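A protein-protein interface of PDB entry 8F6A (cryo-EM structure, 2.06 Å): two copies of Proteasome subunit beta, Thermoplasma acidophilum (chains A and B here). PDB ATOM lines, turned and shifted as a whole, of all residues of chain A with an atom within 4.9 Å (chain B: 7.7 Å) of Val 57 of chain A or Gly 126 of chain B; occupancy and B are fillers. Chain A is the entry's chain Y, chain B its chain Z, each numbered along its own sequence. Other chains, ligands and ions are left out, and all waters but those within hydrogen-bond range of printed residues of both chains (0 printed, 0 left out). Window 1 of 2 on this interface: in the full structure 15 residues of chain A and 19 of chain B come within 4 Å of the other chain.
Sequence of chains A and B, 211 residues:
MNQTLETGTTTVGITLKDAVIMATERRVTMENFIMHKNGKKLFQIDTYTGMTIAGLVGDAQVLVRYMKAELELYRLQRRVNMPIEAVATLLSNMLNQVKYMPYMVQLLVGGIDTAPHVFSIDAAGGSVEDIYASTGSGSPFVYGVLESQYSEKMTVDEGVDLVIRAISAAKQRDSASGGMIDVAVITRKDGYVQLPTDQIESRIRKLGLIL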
ATOM      1  N   VAL A  28      -1.230   8.701 -29.917  1.00  0.00           N
ATOM      2  CA  VAL A  28      -0.695   9.937 -29.349  1.00  0.00           C
ATOM      3  C   VAL A  28      -0.332   9.728 -27.884  1.00  0.00           C
ATOM      4  O   VAL A  28      -1.206   9.698 -27.017  1.00  0.00           O
ATOM      5  CB  VAL A  28      -1.692  11.100 -29.494  1.00  0.00           C
ATOM      6  CG1 VAL A  28      -1.148  12.351 -28.818  1.00  0.00           C
ATOM      7  CG2 VAL A  28      -1.993  11.369 -30.961  1.00  0.00           C
ATOM      8  N   MET A  30       0.701  10.800 -24.303  1.00  0.00           N
ATOM      9  CA  MET A  30       0.677  11.976 -23.448  1.00  0.00           C
ATOM     10  C   MET A  30       0.625  11.524 -21.993  1.00  0.00           C
ATOM     11  O   MET A  30      -0.030  10.533 -21.662  1.00  0.00           O
ATOM     12  CB  MET A  30      -0.505  12.899 -23.810  1.00  0.00           C
ATOM     13  CG  MET A  30      -0.450  14.268 -23.161  1.00  0.00           C
ATOM     14  SD  MET A  30      -1.726  15.417 -23.712  1.00  0.00           S
ATOM     15  CE  MET A  30      -3.170  14.392 -23.785  1.00  0.00           C
ATOM     16  N   GLY A  55       6.596  14.769 -33.444  1.00  0.00           N
ATOM     17  CA  GLY A  55       7.198  15.543 -32.374  1.00  0.00           C
ATOM     18  C   GLY A  55       6.194  16.079 -31.373  1.00  0.00           C
ATOM     19  O   GLY A  55       5.209  15.408 -31.059  1.00  0.00           O
ATOM     20  N   LEU A  56       6.437  17.284 -30.858  1.00  0.00           N
ATOM     21  CA  LEU A  56       5.536  17.884 -29.878  1.00  0.00           C
ATOM     22  C   LEU A  56       4.191  18.197 -30.519  1.00  0.00           C
ATOM     23  O   LEU A  56       4.125  18.898 -31.533  1.00  0.00           O
ATOM     24  CB  LEU A  56       6.159  19.155 -29.299  1.00  0.00           C
ATOM     25  CG  LEU A  56       6.494  19.196 -27.807  1.00  0.00           C
ATOM     26  CD1 LEU A  56       6.930  20.597 -27.407  1.00  0.00           C
ATOM     27  CD2 LEU A  56       5.318  18.740 -26.956  1.00  0.00           C
ATOM     28  N   VAL A  57       3.116  17.687 -29.913  1.00  0.00           N
ATOM     29  CA  VAL A  57       1.781  17.827 -30.494  1.00  0.00           C
ATOM     30  C   VAL A  57       1.378  19.296 -30.564  1.00  0.00           C
ATOM     31  O   VAL A  57       0.894  19.779 -31.595  1.00  0.00           O
ATOM     32  CB  VAL A  57       0.755  17.003 -29.698  1.00  0.00           C
ATOM     33  CG1 VAL A  57      -0.639  17.181 -30.281  1.00  0.00           C
ATOM     34  CG2 VAL A  57       1.150  15.536 -29.692  1.00  0.00           C
ATOM     35  N   GLY A  58       1.585  20.030 -29.468  1.00  0.00           N
ATOM     36  CA  GLY A  58       1.173  21.426 -29.434  1.00  0.00           C
ATOM     37  C   GLY A  58       1.868  22.274 -30.481  1.00  0.00           C
ATOM     38  O   GLY A  58       1.234  23.068 -31.176  1.00  0.00           O
ATOM     39  N   ASP A  59       3.186  22.103 -30.614  1.00  0.00           N
ATOM     40  CA  ASP A  59       3.936  22.829 -31.634  1.00  0.00           C
ATOM     41  C   ASP A  59       3.441  22.478 -33.034  1.00  0.00           C
ATOM     42  O   ASP A  59       3.284  23.355 -33.889  1.00  0.00           O
ATOM     43  CB  ASP A  59       5.429  22.521 -31.501  1.00  0.00           C
ATOM     44  CG  ASP A  59       6.092  23.310 -30.390  1.00  0.00           C
ATOM     45  OD1 ASP A  59       5.399  24.106 -29.727  1.00  0.00           O
ATOM     46  OD2 ASP A  59       7.307  23.125 -30.176  1.00  0.00           O
ATOM     47  N   ALA A  60       3.188  21.190 -33.279  1.00  0.00           N
ATOM     48  CA  ALA A  60       2.776  20.745 -34.606  1.00  0.00           C
ATOM     49  C   ALA A  60       1.402  21.290 -34.981  1.00  0.00           C
ATOM     50  O   ALA A  60       1.186  21.725 -36.117  1.00  0.00           O
ATOM     51  CB  ALA A  60       2.785  19.218 -34.668  1.00  0.00           C
ATOM     52  N   GLN A  61       0.455  21.263 -34.040  1.00  0.00           N
ATOM     53  CA  GLN A  61      -0.894  21.745 -34.337  1.00  0.00           C
ATOM     54  C   GLN A  61      -0.896  23.240 -34.635  1.00  0.00           C
ATOM     55  O   GLN A  61      -1.645  23.704 -35.502  1.00  0.00           O
ATOM     56  CB  GLN A  61      -1.841  21.415 -33.181  1.00  0.00           C
ATOM     57  CG  GLN A  61      -1.963  19.921 -32.891  1.00  0.00           C
ATOM     58  CD  GLN A  61      -2.960  19.599 -31.791  1.00  0.00           C
ATOM     59  OE1 GLN A  61      -3.008  20.268 -30.761  1.00  0.00           O
ATOM     60  NE2 GLN A  61      -3.754  18.561 -32.005  1.00  0.00           N
ATOM     61  N   ALA B  88     -11.240  24.583 -27.428  1.00  0.00           N
ATOM     62  CA  ALA B  88      -9.968  23.879 -27.293  1.00  0.00           C
ATOM     63  C   ALA B  88      -8.866  24.575 -28.084  1.00  0.00           C
ATOM     64  O   ALA B  88      -7.735  24.705 -27.607  1.00  0.00           O
ATOM     65  CB  ALA B  88     -10.124  22.425 -27.743  1.00  0.00           C
ATOM     66  N   LEU B  91      -7.619  27.705 -26.304  1.00  0.00           N
ATOM     67  CA  LEU B  91      -6.754  27.308 -25.198  1.00  0.00           C
ATOM     68  C   LEU B  91      -5.389  26.864 -25.701  1.00  0.00           C
ATOM     69  O   LEU B  91      -4.355  27.202 -25.114  1.00  0.00           O
ATOM     70  CB  LEU B  91      -7.412  26.185 -24.402  1.00  0.00           C
ATOM     71  CG  LEU B  91      -8.094  26.560 -23.096  1.00  0.00           C
ATOM     72  CD1 LEU B  91      -8.968  25.408 -22.647  1.00  0.00           C
ATOM     73  CD2 LEU B  91      -7.065  26.920 -22.036  1.00  0.00           C
ATOM     74  N   SER B  92      -5.371  26.102 -26.795  1.00  0.00           N
ATOM     75  CA  SER B  92      -4.116  25.593 -27.333  1.00  0.00           C
ATOM     76  C   SER B  92      -3.188  26.733 -27.737  1.00  0.00           C
ATOM     77  O   SER B  92      -1.983  26.693 -27.465  1.00  0.00           O
ATOM     78  CB  SER B  92      -4.406  24.672 -28.521  1.00  0.00           C
ATOM     79  OG  SER B  92      -3.390  24.755 -29.500  1.00  0.00           O
ATOM     80  N   ASN B  93      -3.737  27.770 -28.375  1.00  0.00           N
ATOM     81  CA  ASN B  93      -2.922  28.908 -28.784  1.00  0.00           C
ATOM     82  C   ASN B  93      -2.326  29.636 -27.580  1.00  0.00           C
ATOM     83  O   ASN B  93      -1.138  29.977 -27.579  1.00  0.00           O
ATOM     84  CB  ASN B  93      -3.751  29.866 -29.643  1.00  0.00           C
ATOM     85  CG  ASN B  93      -3.960  29.345 -31.053  1.00  0.00           C
ATOM     86  OD1 ASN B  93      -3.044  28.799 -31.663  1.00  0.00           O
ATOM     87  ND2 ASN B  93      -5.169  29.501 -31.571  1.00  0.00           N
ATOM     88  N   LEU B  95      -1.722  28.548 -24.454  1.00  0.00           N
ATOM     89  CA  LEU B  95      -0.706  27.759 -23.763  1.00  0.00           C
ATOM     90  C   LEU B  95       0.584  27.673 -24.574  1.00  0.00           C
ATOM     91  O   LEU B  95       1.683  27.810 -24.027  1.00  0.00           O
ATOM     92  CB  LEU B  95      -1.244  26.363 -23.452  1.00  0.00           C
ATOM     93  CG  LEU B  95      -2.311  26.317 -22.356  1.00  0.00           C
ATOM     94  CD1 LEU B  95      -3.122  25.036 -22.434  1.00  0.00           C
ATOM     95  CD2 LEU B  95      -1.675  26.468 -20.991  1.00  0.00           C
ATOM     96  N   ASN B  96       0.468  27.451 -25.886  1.00  0.00           N
ATOM     97  CA  ASN B  96       1.664  27.299 -26.710  1.00  0.00           C
ATOM     98  C   ASN B  96       2.447  28.601 -26.804  1.00  0.00           C
ATOM     99  O   ASN B  96       3.678  28.584 -26.926  1.00  0.00           O
ATOM    100  CB  ASN B  96       1.294  26.802 -28.107  1.00  0.00           C
ATOM    101  CG  ASN B  96       2.509  26.373 -28.913  1.00  0.00           C
ATOM    102  OD1 ASN B  96       3.049  27.150 -29.697  1.00  0.00           O
ATOM    103  ND2 ASN B  96       2.948  25.135 -28.719  1.00  0.00           N
ATOM    104  N   LEU B 107      -5.617  20.053 -18.713  1.00  0.00           N
ATOM    105  CA  LEU B 107      -7.002  20.497 -18.758  1.00  0.00           C
ATOM    106  C   LEU B 107      -7.870  19.522 -19.540  1.00  0.00           C
ATOM    107  O   LEU B 107      -7.402  18.835 -20.452  1.00  0.00           O
ATOM    108  CB  LEU B 107      -7.115  21.891 -19.388  1.00  0.00           C
ATOM    109  CG  LEU B 107      -6.184  22.972 -18.835  1.00  0.00           C
ATOM    110  CD1 LEU B 107      -6.123  24.166 -19.768  1.00  0.00           C
ATOM    111  CD2 LEU B 107      -6.620  23.392 -17.442  1.00  0.00           C
ATOM    112  N   PHE B 119     -12.247  17.213 -24.955  1.00  0.00           N
ATOM    113  CA  PHE B 119     -10.910  17.535 -25.438  1.00  0.00           C
ATOM    114  C   PHE B 119      -9.921  17.499 -24.282  1.00  0.00           C
ATOM    115  O   PHE B 119     -10.233  17.955 -23.179  1.00  0.00           O
ATOM    116  CB  PHE B 119     -10.871  18.916 -26.103  1.00  0.00           C
ATOM    117  CG  PHE B 119     -11.427  18.941 -27.496  1.00  0.00           C
ATOM    118  CD1 PHE B 119     -12.784  19.113 -27.712  1.00  0.00           C
ATOM    119  CD2 PHE B 119     -10.591  18.800 -28.593  1.00  0.00           C
ATOM    120  CE1 PHE B 119     -13.298  19.140 -28.997  1.00  0.00           C
ATOM    121  CE2 PHE B 119     -11.099  18.827 -29.878  1.00  0.00           C
ATOM    122  CZ  PHE B 119     -12.456  18.996 -30.080  1.00  0.00           C
ATOM    123  N   SER B 120      -8.733  16.961 -24.541  1.00  0.00           N
ATOM    124  CA  SER B 120      -7.636  16.965 -23.583  1.00  0.00           C
ATOM    125  C   SER B 120      -6.541  17.897 -24.083  1.00  0.00           C
ATOM    126  O   SER B 120      -6.114  17.793 -25.237  1.00  0.00           O
ATOM    127  CB  SER B 120      -7.090  15.552 -23.378  1.00  0.00           C
ATOM    128  OG  SER B 120      -5.755  15.578 -22.922  1.00  0.00           O
ATOM    129  N   ILE B 121      -6.090  18.805 -23.220  1.00  0.00           N
ATOM    130  CA  ILE B 121      -5.099  19.814 -23.579  1.00  0.00           C
ATOM    131  C   ILE B 121      -3.974  19.786 -22.551  1.00  0.00           C
ATOM    132  O   ILE B 121      -4.231  19.818 -21.344  1.00  0.00           O
ATOM    133  CB  ILE B 121      -5.716  21.224 -23.668  1.00  0.00           C
ATOM    134  CG1 ILE B 121      -6.889  21.254 -24.655  1.00  0.00           C
ATOM    135  CG2 ILE B 121      -4.672  22.235 -24.090  1.00  0.00           C
ATOM    136  CD1 ILE B 121      -8.247  21.144 -24.010  1.00  0.00           C
ATOM    137  N   ASP B 122      -2.730  19.733 -23.028  1.00  0.00           N
ATOM    138  CA  ASP B 122      -1.566  19.686 -22.157  1.00  0.00           C
ATOM    139  C   ASP B 122      -0.943  21.074 -22.009  1.00  0.00           C
ATOM    140  O   ASP B 122      -1.401  22.059 -22.589  1.00  0.00           O
ATOM    141  CB  ASP B 122      -0.542  18.662 -22.663  1.00  0.00           C
ATOM    142  CG  ASP B 122      -0.010  18.976 -24.062  1.00  0.00           C
ATOM    143  OD1 ASP B 122       0.265  20.148 -24.384  1.00  0.00           O
ATOM    144  OD2 ASP B 122       0.140  18.025 -24.853  1.00  0.00           O
ATOM    145  N   ALA B 123       0.145  21.132 -21.235  1.00  0.00           N
ATOM    146  CA  ALA B 123       0.764  22.408 -20.898  1.00  0.00           C
ATOM    147  C   ALA B 123       1.370  23.098 -22.114  1.00  0.00           C
ATOM    148  O   ALA B 123       1.476  24.328 -22.136  1.00  0.00           O
ATOM    149  CB  ALA B 123       1.831  22.200 -19.822  1.00  0.00           C
ATOM    150  N   ALA B 124       1.770  22.336 -23.131  1.00  0.00           N
ATOM    151  CA  ALA B 124       2.395  22.895 -24.322  1.00  0.00           C
ATOM    152  C   ALA B 124       1.386  23.232 -25.416  1.00  0.00           C
ATOM    153  O   ALA B 124       1.787  23.596 -26.526  1.00  0.00           O
ATOM    154  CB  ALA B 124       3.459  21.937 -24.862  1.00  0.00           C
ATOM    155  N   GLY B 125       0.091  23.117 -25.133  1.00  0.00           N
ATOM    156  CA  GLY B 125      -0.923  23.446 -26.110  1.00  0.00           C
ATOM    157  C   GLY B 125      -1.365  22.314 -27.010  1.00  0.00           C
ATOM    158  O   GLY B 125      -2.173  22.549 -27.912  1.00  0.00           O
ATOM    159  N   GLY B 126      -0.859  21.101 -26.813  1.00  0.00           N
ATOM    160  CA  GLY B 126      -1.357  19.965 -27.563  1.00  0.00           C
ATOM    161  C   GLY B 126      -2.798  19.646 -27.216  1.00  0.00           C
ATOM    162  O   GLY B 126      -3.119  19.442 -26.043  1.00  0.00           O
ATOM    163  N   SER B 127      -3.676  19.600 -28.216  1.00  0.00           N
ATOM    164  CA  SER B 127      -5.103  19.383 -27.997  1.00  0.00           C
ATOM    165  C   SER B 127      -5.568  18.201 -28.836  1.00  0.00           C
ATOM    166  O   SER B 127      -5.359  18.185 -30.052  1.00  0.00           O
ATOM    167  CB  SER B 127      -5.906  20.639 -28.341  1.00  0.00           C
ATOM    168  OG  SER B 127      -7.297  20.391 -28.262  1.00  0.00           O
ATOM    169  N   VAL B 128      -6.196  17.219 -28.190  1.00  0.00           N
ATOM    170  CA  VAL B 128      -6.658  16.004 -28.860  1.00  0.00           C
ATOM    171  C   VAL B 128      -8.072  15.685 -28.387  1.00  0.00           C
ATOM    172  O   VAL B 128      -8.325  15.632 -27.179  1.00  0.00           O
ATOM    173  CB  VAL B 128      -5.733  14.801 -28.595  1.00  0.00           C
ATOM    174  CG1 VAL B 128      -6.261  13.561 -29.299  1.00  0.00           C
ATOM    175  CG2 VAL B 128      -4.309  15.106 -29.033  1.00  0.00           C
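Val 57 of chain A touches one residue of chain B. Gly 126 of chain B touches three residues of chain A. Gly 58 of chain A touches just these residues of chain B: Asn 96 (3.5 Å), Ala 124 (3.7 Å), Gly 125 (3.6 Å) and Gly 126 (3.3 Å). Of the printed residues of chain A, Gly 125 of chain B touches Gly 58 (3.6 Å) and Gln 61 (3.7 Å). Of the printed residues of chain B, Gln 61 of chain A touches Gly 125, Gly 126 and Ser 127. Val 28 of chain A touches none of the printed residues of chain B. The nearest printed residue of chain B that does not touch Val 57 of chain A is Val 128 of chain B (4.4 Å). The nearest printed residue of chain A that does not touch Gly 126 of chain B is Met 30 of chain A (4.9 Å).
No position is printed for both chains. Of the 11 pairs that touch across the chains among the printed residues, none has its exchanged pair printed and touching as well.
Among the printed residues, merely in contact across the chains: Met 30 of chain A with Ser 120 of chain B, Val 57 of chain A with Gly 126 of chain B, Gly 58 of chain A with Asn 96 of chain B, Gly 58 of chain A with Ala 124 of chain B, Gly 58 of chain A with Gly 125 of chain B, Gly 58 of chain A with Gly 126 of chain B, Gln 61 of chain A with Gly 125 of chain B and Gln 61 of chain A with Gly 126 of chain B.
ND2 of Asn 96 of chain B is in hydrogen-bond range of OD1 of Asp 59 of chain A (2.8 Å). The side-chain amide nitrogen of Gln 61 of chain A is in hydrogen-bond range of the backbone carbonyl oxygen of Ser 127 of chain B, at 2.6 Å. The side-chain sulfur (SD) of Met 30 of chain A sits close to the side-chain carboxylate (OD2) of Asp 122 of chain B.
OG of Ser 92 of chain B lies within hydrogen-bond range of O of Gly 125 of chain B, at 3.0 Å. OD1 of Asp 122 of chain B lies within hydrogen-bond range of N of Gly 126 of chain B. The backbone NH of Ser 120 of chain B is in hydrogen-bond range of the backbone carbonyl oxygen of Val 128 of chain B, at 3.0 Å. OD1 of Asp 122 of chain B sits at hydrogen-bond distance from N of Gly 125 of chain B (3.1 Å). N of Ala 124 of chain B is in hydrogen-bond range of OD1 of Asp 122 of chain B (2.9 Å). The backbone carbonyl oxygen (O) of Ala 124 of chain B lies within hydrogen-bond range of the side-chain amide nitrogen (ND2) of Asn 96 of chain B, at 2.9 Å.
Printed residues of chain A that touch a printed residue of chain B: Met 30, Val 57, Gly 58, Asp 59 and Gln 61. Hydrophobic or aromatic side chains of chain A within 4 Å of the printed part of chain B: Met 30 and Val 57. Among the printed residues, 11 pairs touch across the chains. Among the printed residues, no Asp or Glu carboxylate lies within 4 Å of a Lys or Arg side-chain nitrogen of the other chain.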
